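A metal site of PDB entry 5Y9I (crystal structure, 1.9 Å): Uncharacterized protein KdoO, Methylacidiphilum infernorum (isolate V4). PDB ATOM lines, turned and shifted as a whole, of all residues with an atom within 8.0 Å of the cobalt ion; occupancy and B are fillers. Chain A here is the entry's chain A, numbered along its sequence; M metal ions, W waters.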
ATOM      1  N   ASP A 142      18.091 -13.678   2.127  1.00  0.00           N
ATOM      2  CA  ASP A 142      16.968 -12.847   2.542  1.00  0.00           C
ATOM      3  C   ASP A 142      16.778 -11.602   1.679  1.00  0.00           C
ATOM      4  O   ASP A 142      15.994 -10.729   2.059  1.00  0.00           O
ATOM      5  CB  ASP A 142      17.104 -12.483   4.025  1.00  0.00           C
ATOM      6  CG  ASP A 142      16.648 -13.617   4.940  1.00  0.00           C
ATOM      7  OD1 ASP A 142      16.142 -14.667   4.439  1.00  0.00           O
ATOM      8  OD2 ASP A 142      16.780 -13.475   6.171  1.00  0.00           O
ATOM      9  N   ARG A 144      15.378 -12.464  -0.943  1.00  0.00           N
ATOM     10  CA  ARG A 144      14.200 -13.107  -1.519  1.00  0.00           C
ATOM     11  C   ARG A 144      13.048 -12.992  -0.515  1.00  0.00           C
ATOM     12  O   ARG A 144      13.251 -13.214   0.679  1.00  0.00           O
ATOM     13  CB  ARG A 144      14.494 -14.578  -1.829  1.00  0.00           C
ATOM     14  CG  ARG A 144      15.548 -14.803  -2.910  1.00  0.00           C
ATOM     15  CD  ARG A 144      16.012 -16.261  -2.949  1.00  0.00           C
ATOM     16  NE  ARG A 144      17.208 -16.437  -3.771  1.00  0.00           N
ATOM     17  CZ  ARG A 144      17.296 -17.240  -4.835  1.00  0.00           C
ATOM     18  NH1 ARG A 144      16.250 -17.974  -5.224  1.00  0.00           N
ATOM     19  NH2 ARG A 144      18.441 -17.314  -5.507  1.00  0.00           N
ATOM     20  N   LEU A 145      11.869 -12.620  -1.004  1.00  0.00           N
ATOM     21  CA  LEU A 145      10.716 -12.441  -0.135  1.00  0.00           C
ATOM     22  C   LEU A 145      10.378 -13.729   0.596  1.00  0.00           C
ATOM     23  O   LEU A 145      10.325 -14.803  -0.012  1.00  0.00           O
ATOM     24  CB  LEU A 145       9.484 -11.993  -0.935  1.00  0.00           C
ATOM     25  CG  LEU A 145       9.505 -10.600  -1.564  1.00  0.00           C
ATOM     26  CD1 LEU A 145       8.473 -10.513  -2.691  1.00  0.00           C
ATOM     27  CD2 LEU A 145       9.253  -9.546  -0.487  1.00  0.00           C
ATOM     28  N   HIS A 146      10.094 -13.616   1.892  1.00  0.00           N
ATOM     29  CA  HIS A 146       9.782 -14.772   2.708  1.00  0.00           C
ATOM     30  C   HIS A 146       9.006 -14.311   3.940  1.00  0.00           C
ATOM     31  O   HIS A 146       9.012 -13.121   4.278  1.00  0.00           O
ATOM     32  CB  HIS A 146      11.062 -15.467   3.155  1.00  0.00           C
ATOM     33  CG  HIS A 146      11.934 -14.593   4.003  1.00  0.00           C
ATOM     34  ND1 HIS A 146      12.766 -13.639   3.453  1.00  0.00           N
ATOM     35  CD2 HIS A 146      12.029 -14.455   5.343  1.00  0.00           C
ATOM     36  CE1 HIS A 146      13.367 -12.969   4.427  1.00  0.00           C
ATOM     37  NE2 HIS A 146      12.929 -13.435   5.583  1.00  0.00           N
ATOM     38  N   VAL A 147       8.350 -15.267   4.595  1.00  0.00           N
ATOM     39  CA  VAL A 147       7.993 -15.130   6.002  1.00  0.00           C
ATOM     40  C   VAL A 147       9.041 -15.900   6.789  1.00  0.00           C
ATOM     41  O   VAL A 147       9.701 -16.817   6.280  1.00  0.00           O
ATOM     42  CB  VAL A 147       6.567 -15.624   6.337  1.00  0.00           C
ATOM     43  CG1 VAL A 147       5.491 -14.784   5.636  1.00  0.00           C
ATOM     44  CG2 VAL A 147       6.417 -17.101   5.985  1.00  0.00           C
ATOM     45  N   ASP A 148       9.209 -15.544   8.060  1.00  0.00           N
ATOM     46  CA  ASP A 148      10.247 -16.156   8.876  1.00  0.00           C
ATOM     47  C   ASP A 148       9.851 -17.554   9.326  1.00  0.00           C
ATOM     48  O   ASP A 148       8.762 -17.772   9.860  1.00  0.00           O
ATOM     49  CB  ASP A 148      10.566 -15.308  10.099  1.00  0.00           C
ATOM     50  CG  ASP A 148      11.384 -14.081   9.752  1.00  0.00           C
ATOM     51  OD1 ASP A 148      11.760 -13.928   8.570  1.00  0.00           O
ATOM     52  OD2 ASP A 148      11.645 -13.287  10.673  1.00  0.00           O
ATOM     53  N   ALA A 149      10.772 -18.498   9.124  1.00  0.00           N
ATOM     54  CA  ALA A 149      10.666 -19.853   9.622  1.00  0.00           C
ATOM     55  C   ALA A 149      12.085 -20.385   9.716  1.00  0.00           C
ATOM     56  O   ALA A 149      12.851 -20.210   8.765  1.00  0.00           O
ATOM     57  CB  ALA A 149       9.802 -20.721   8.702  1.00  0.00           C
ATOM     58  N   PHE A 150      12.448 -20.979  10.840  1.00  0.00           N
ATOM     59  CA  PHE A 150      13.825 -21.391  11.061  1.00  0.00           C
ATOM     60  C   PHE A 150      13.869 -22.896  11.279  1.00  0.00           C
ATOM     61  O   PHE A 150      13.217 -23.399  12.215  1.00  0.00           O
ATOM     62  CB  PHE A 150      14.412 -20.634  12.256  1.00  0.00           C
ATOM     63  CG  PHE A 150      14.253 -19.142  12.127  1.00  0.00           C
ATOM     64  CD1 PHE A 150      15.065 -18.415  11.263  1.00  0.00           C
ATOM     65  CD2 PHE A 150      13.279 -18.474  12.831  1.00  0.00           C
ATOM     66  CE1 PHE A 150      14.912 -17.046  11.115  1.00  0.00           C
ATOM     67  CE2 PHE A 150      13.122 -17.104  12.697  1.00  0.00           C
ATOM     68  CZ  PHE A 150      13.947 -16.394  11.846  1.00  0.00           C
ATOM     69  N   ARG A 162       8.839  -9.001  15.805  1.00  0.00           N
ATOM     70  CA  ARG A 162      10.179  -8.418  15.842  1.00  0.00           C
ATOM     71  C   ARG A 162      10.144  -6.893  15.829  1.00  0.00           C
ATOM     72  O   ARG A 162       9.347  -6.281  15.121  1.00  0.00           O
ATOM     73  CB  ARG A 162      11.023  -8.964  14.682  1.00  0.00           C
ATOM     74  CG  ARG A 162      11.408 -10.427  14.954  1.00  0.00           C
ATOM     75  CD  ARG A 162      12.266 -11.056  13.861  1.00  0.00           C
ATOM     76  NE  ARG A 162      13.176 -12.031  14.456  1.00  0.00           N
ATOM     77  CZ  ARG A 162      14.115 -12.692  13.794  1.00  0.00           C
ATOM     78  NH1 ARG A 162      14.258 -12.532  12.491  1.00  0.00           N
ATOM     79  NH2 ARG A 162      14.903 -13.543  14.443  1.00  0.00           N
ATOM     80  N   PHE A 164      12.719  -3.628  15.184  1.00  0.00           N
ATOM     81  CA  PHE A 164      13.944  -3.310  14.444  1.00  0.00           C
ATOM     82  C   PHE A 164      14.280  -1.844  14.677  1.00  0.00           C
ATOM     83  O   PHE A 164      13.386  -0.991  14.640  1.00  0.00           O
ATOM     84  CB  PHE A 164      13.776  -3.538  12.928  1.00  0.00           C
ATOM     85  CG  PHE A 164      13.450  -4.956  12.530  1.00  0.00           C
ATOM     86  CD1 PHE A 164      12.132  -5.395  12.502  1.00  0.00           C
ATOM     87  CD2 PHE A 164      14.445  -5.828  12.123  1.00  0.00           C
ATOM     88  CE1 PHE A 164      11.815  -6.696  12.113  1.00  0.00           C
ATOM     89  CE2 PHE A 164      14.144  -7.126  11.716  1.00  0.00           C
ATOM     90  CZ  PHE A 164      12.824  -7.563  11.725  1.00  0.00           C
ATOM     91  N   TRP A 176      14.203  -2.364   2.570  1.00  0.00           N
ATOM     92  CA  TRP A 176      13.336  -3.528   2.579  1.00  0.00           C
ATOM     93  C   TRP A 176      12.454  -3.544   1.343  1.00  0.00           C
ATOM     94  O   TRP A 176      12.221  -2.519   0.704  1.00  0.00           O
ATOM     95  CB  TRP A 176      12.411  -3.538   3.806  1.00  0.00           C
ATOM     96  CG  TRP A 176      12.989  -4.119   5.065  1.00  0.00           C
ATOM     97  CD1 TRP A 176      14.277  -4.069   5.489  1.00  0.00           C
ATOM     98  CD2 TRP A 176      12.251  -4.835   6.065  1.00  0.00           C
ATOM     99  NE1 TRP A 176      14.398  -4.716   6.712  1.00  0.00           N
ATOM    100  CE2 TRP A 176      13.173  -5.193   7.074  1.00  0.00           C
ATOM    101  CE3 TRP A 176      10.908  -5.216   6.200  1.00  0.00           C
ATOM    102  CZ2 TRP A 176      12.792  -5.917   8.213  1.00  0.00           C
ATOM    103  CZ3 TRP A 176      10.535  -5.933   7.325  1.00  0.00           C
ATOM    104  CH2 TRP A 176      11.476  -6.278   8.316  1.00  0.00           C
ATOM    105  N   HIS A 225       8.325 -20.724   3.183  1.00  0.00           N
ATOM    106  CA  HIS A 225       9.579 -19.992   3.169  1.00  0.00           C
ATOM    107  C   HIS A 225      10.481 -20.456   2.022  1.00  0.00           C
ATOM    108  O   HIS A 225      10.907 -19.649   1.186  1.00  0.00           O
ATOM    109  CB  HIS A 225      10.275 -20.176   4.524  1.00  0.00           C
ATOM    110  CG  HIS A 225      11.647 -19.585   4.626  1.00  0.00           C
ATOM    111  ND1 HIS A 225      12.773 -20.220   4.149  1.00  0.00           N
ATOM    112  CD2 HIS A 225      12.075 -18.442   5.198  1.00  0.00           C
ATOM    113  CE1 HIS A 225      13.837 -19.485   4.403  1.00  0.00           C
ATOM    114  NE2 HIS A 225      13.447 -18.394   5.055  1.00  0.00           N
ATOM    115  N   LYS A 229      10.936 -18.764  -1.907  1.00  0.00           N
ATOM    116  CA  LYS A 229      12.227 -18.219  -2.299  1.00  0.00           C
ATOM    117  C   LYS A 229      12.699 -18.795  -3.632  1.00  0.00           C
ATOM    118  O   LYS A 229      13.372 -18.090  -4.397  1.00  0.00           O
ATOM    119  CB  LYS A 229      13.259 -18.483  -1.199  1.00  0.00           C
ATOM    120  CG  LYS A 229      13.137 -17.521  -0.003  1.00  0.00           C
ATOM    121  CD  LYS A 229      14.383 -17.600   0.848  1.00  0.00           C
ATOM    122  CE  LYS A 229      14.398 -16.558   1.959  1.00  0.00           C
ATOM    123  NZ  LYS A 229      15.721 -16.587   2.690  1.00  0.00           N
ATOM    124  N   THR A 255       6.958 -10.982  11.629  1.00  0.00           N
ATOM    125  CA  THR A 255       7.737 -11.377  10.455  1.00  0.00           C
ATOM    126  C   THR A 255       7.387 -12.775   9.960  1.00  0.00           C
ATOM    127  O   THR A 255       7.863 -13.162   8.883  1.00  0.00           O
ATOM    128  CB  THR A 255       9.229 -11.302  10.760  1.00  0.00           C
ATOM    129  OG1 THR A 255       9.529 -12.120  11.890  1.00  0.00           O
ATOM    130  CG2 THR A 255       9.653  -9.853  11.047  1.00  0.00           C
ATOM    131  N   ASP A 256       6.585 -13.541  10.707  1.00  0.00           N
ATOM    132  CA  ASP A 256       6.028 -14.788  10.189  1.00  0.00           C
ATOM    133  C   ASP A 256       4.787 -14.568   9.321  1.00  0.00           C
ATOM    134  O   ASP A 256       4.228 -15.550   8.804  1.00  0.00           O
ATOM    135  CB  ASP A 256       5.682 -15.716  11.356  1.00  0.00           C
ATOM    136  CG  ASP A 256       4.677 -15.097  12.316  1.00  0.00           C
ATOM    137  OD1 ASP A 256       4.275 -13.923  12.137  1.00  0.00           O
ATOM    138  OD2 ASP A 256       4.281 -15.806  13.272  1.00  0.00           O
ATOM    139  N   VAL A 258       4.228 -11.050   7.545  1.00  0.00           N
ATOM    140  CA  VAL A 258       4.553 -10.023   6.558  1.00  0.00           C
ATOM    141  C   VAL A 258       5.677 -10.530   5.666  1.00  0.00           C
ATOM    142  O   VAL A 258       6.783 -10.803   6.145  1.00  0.00           O
ATOM    143  CB  VAL A 258       4.967  -8.708   7.244  1.00  0.00           C
ATOM    144  CG1 VAL A 258       5.322  -7.640   6.193  1.00  0.00           C
ATOM    145  CG2 VAL A 258       3.840  -8.221   8.167  1.00  0.00           C
ATOM    146  N   LEU A 259       5.387 -10.677   4.365  1.00  0.00           N
ATOM    147  CA  LEU A 259       6.424 -11.035   3.401  1.00  0.00           C
ATOM    148  C   LEU A 259       7.427  -9.912   3.314  1.00  0.00           C
ATOM    149  O   LEU A 259       7.052  -8.762   3.094  1.00  0.00           O
ATOM    150  CB  LEU A 259       5.804 -11.261   2.009  1.00  0.00           C
ATOM    151  CG  LEU A 259       5.229 -12.609   1.626  1.00  0.00           C
ATOM    152  CD1 LEU A 259       4.013 -12.940   2.495  1.00  0.00           C
ATOM    153  CD2 LEU A 259       4.878 -12.597   0.140  1.00  0.00           C
ATOM    154  N   HIS A 260       8.709 -10.226   3.491  1.00  0.00           N
ATOM    155  CA  HIS A 260       9.718  -9.183   3.498  1.00  0.00           C
ATOM    156  C   HIS A 260      10.999  -9.693   2.868  1.00  0.00           C
ATOM    157  O   HIS A 260      11.226 -10.900   2.741  1.00  0.00           O
ATOM    158  CB  HIS A 260       9.984  -8.693   4.932  1.00  0.00           C
ATOM    159  CG  HIS A 260      10.411  -9.793   5.844  1.00  0.00           C
ATOM    160  ND1 HIS A 260       9.528 -10.678   6.402  1.00  0.00           N
ATOM    161  CD2 HIS A 260      11.649 -10.182   6.255  1.00  0.00           C
ATOM    162  CE1 HIS A 260      10.192 -11.559   7.141  1.00  0.00           C
ATOM    163  NE2 HIS A 260      11.479 -11.284   7.056  1.00  0.00           N
ATOM    164  N   ALA A 261      11.858  -8.750   2.495  1.00  0.00           N
ATOM    165  CA  ALA A 261      13.187  -9.028   1.972  1.00  0.00           C
ATOM    166  C   ALA A 261      14.052  -7.826   2.326  1.00  0.00           C
ATOM    167  O   ALA A 261      13.535  -6.716   2.464  1.00  0.00           O
ATOM    168  CB  ALA A 261      13.174  -9.261   0.445  1.00  0.00           C
ATOM    169  N   VAL A 262      15.344  -8.056   2.516  1.00  0.00           N
ATOM    170  CA  VAL A 262      16.278  -6.995   2.884  1.00  0.00           C
ATOM    171  C   VAL A 262      17.349  -6.864   1.805  1.00  0.00           C
ATOM    172  O   VAL A 262      18.049  -7.840   1.512  1.00  0.00           O
ATOM    173  CB  VAL A 262      16.929  -7.246   4.258  1.00  0.00           C
ATOM    174  CG1 VAL A 262      17.593  -5.960   4.754  1.00  0.00           C
ATOM    175  CG2 VAL A 262      15.891  -7.757   5.249  1.00  0.00           C
ATOM    176  N   GLU A 270      17.829  -5.602  16.813  1.00  0.00           N
ATOM    177  CA  GLU A 270      16.645  -6.392  16.528  1.00  0.00           C
ATOM    178  C   GLU A 270      16.264  -7.159  17.783  1.00  0.00           C
ATOM    179  O   GLU A 270      17.130  -7.682  18.476  1.00  0.00           O
ATOM    180  CB  GLU A 270      16.923  -7.360  15.366  1.00  0.00           C
ATOM    181  CG  GLU A 270      15.776  -8.246  14.927  1.00  0.00           C
ATOM    182  CD  GLU A 270      16.143  -9.037  13.668  1.00  0.00           C
ATOM    183  OE1 GLU A 270      17.235  -8.809  13.112  1.00  0.00           O
ATOM    184  OE2 GLU A 270      15.327  -9.888  13.230  1.00  0.00           O
HETATM  185 CO    CO M   1      13.097 -12.542   7.541  1.00  0.00          CO
HETATM  186  O   HOH W   1      14.673 -11.251   6.816  1.00  0.00           O
HETATM  187  O   HOH W   2      13.364 -11.607   9.403  1.00  0.00           O
HETATM  188  O   HOH W   3      14.702 -14.068   8.088  1.00  0.00           O
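Water W2 bridges OD2 of Asp 148 and NH1 of Arg 162.
The nearest printed residue that does not touch the cobalt ion is Asp 142 (4.04 Å).
The cobalt ion is bound by water W2, a ring nitrogen (NE2) of His 260, a ring nitrogen (NE2) of His 146, water W1, the side-chain carboxylate of Asp 148 and water W3.
A ring nitrogen (ND1) of His 146 lies within hydrogen-bond range of the backbone carbonyl oxygen of Arg 144, at 2.8 Å. ND1 of His 260 lies within hydrogen-bond range of O of Val 258 (2.8 Å). The guanidinium group (NH1) of Arg 162 lies within salt-bridge range of the side-chain carboxylate (OD2) of Asp 148 (3.3 Å). The side-chain hydroxyl (OG1) of Thr 255 lies within hydrogen-bond range of the side-chain carboxylate (OD2) of Asp 148, at 2.7 Å.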
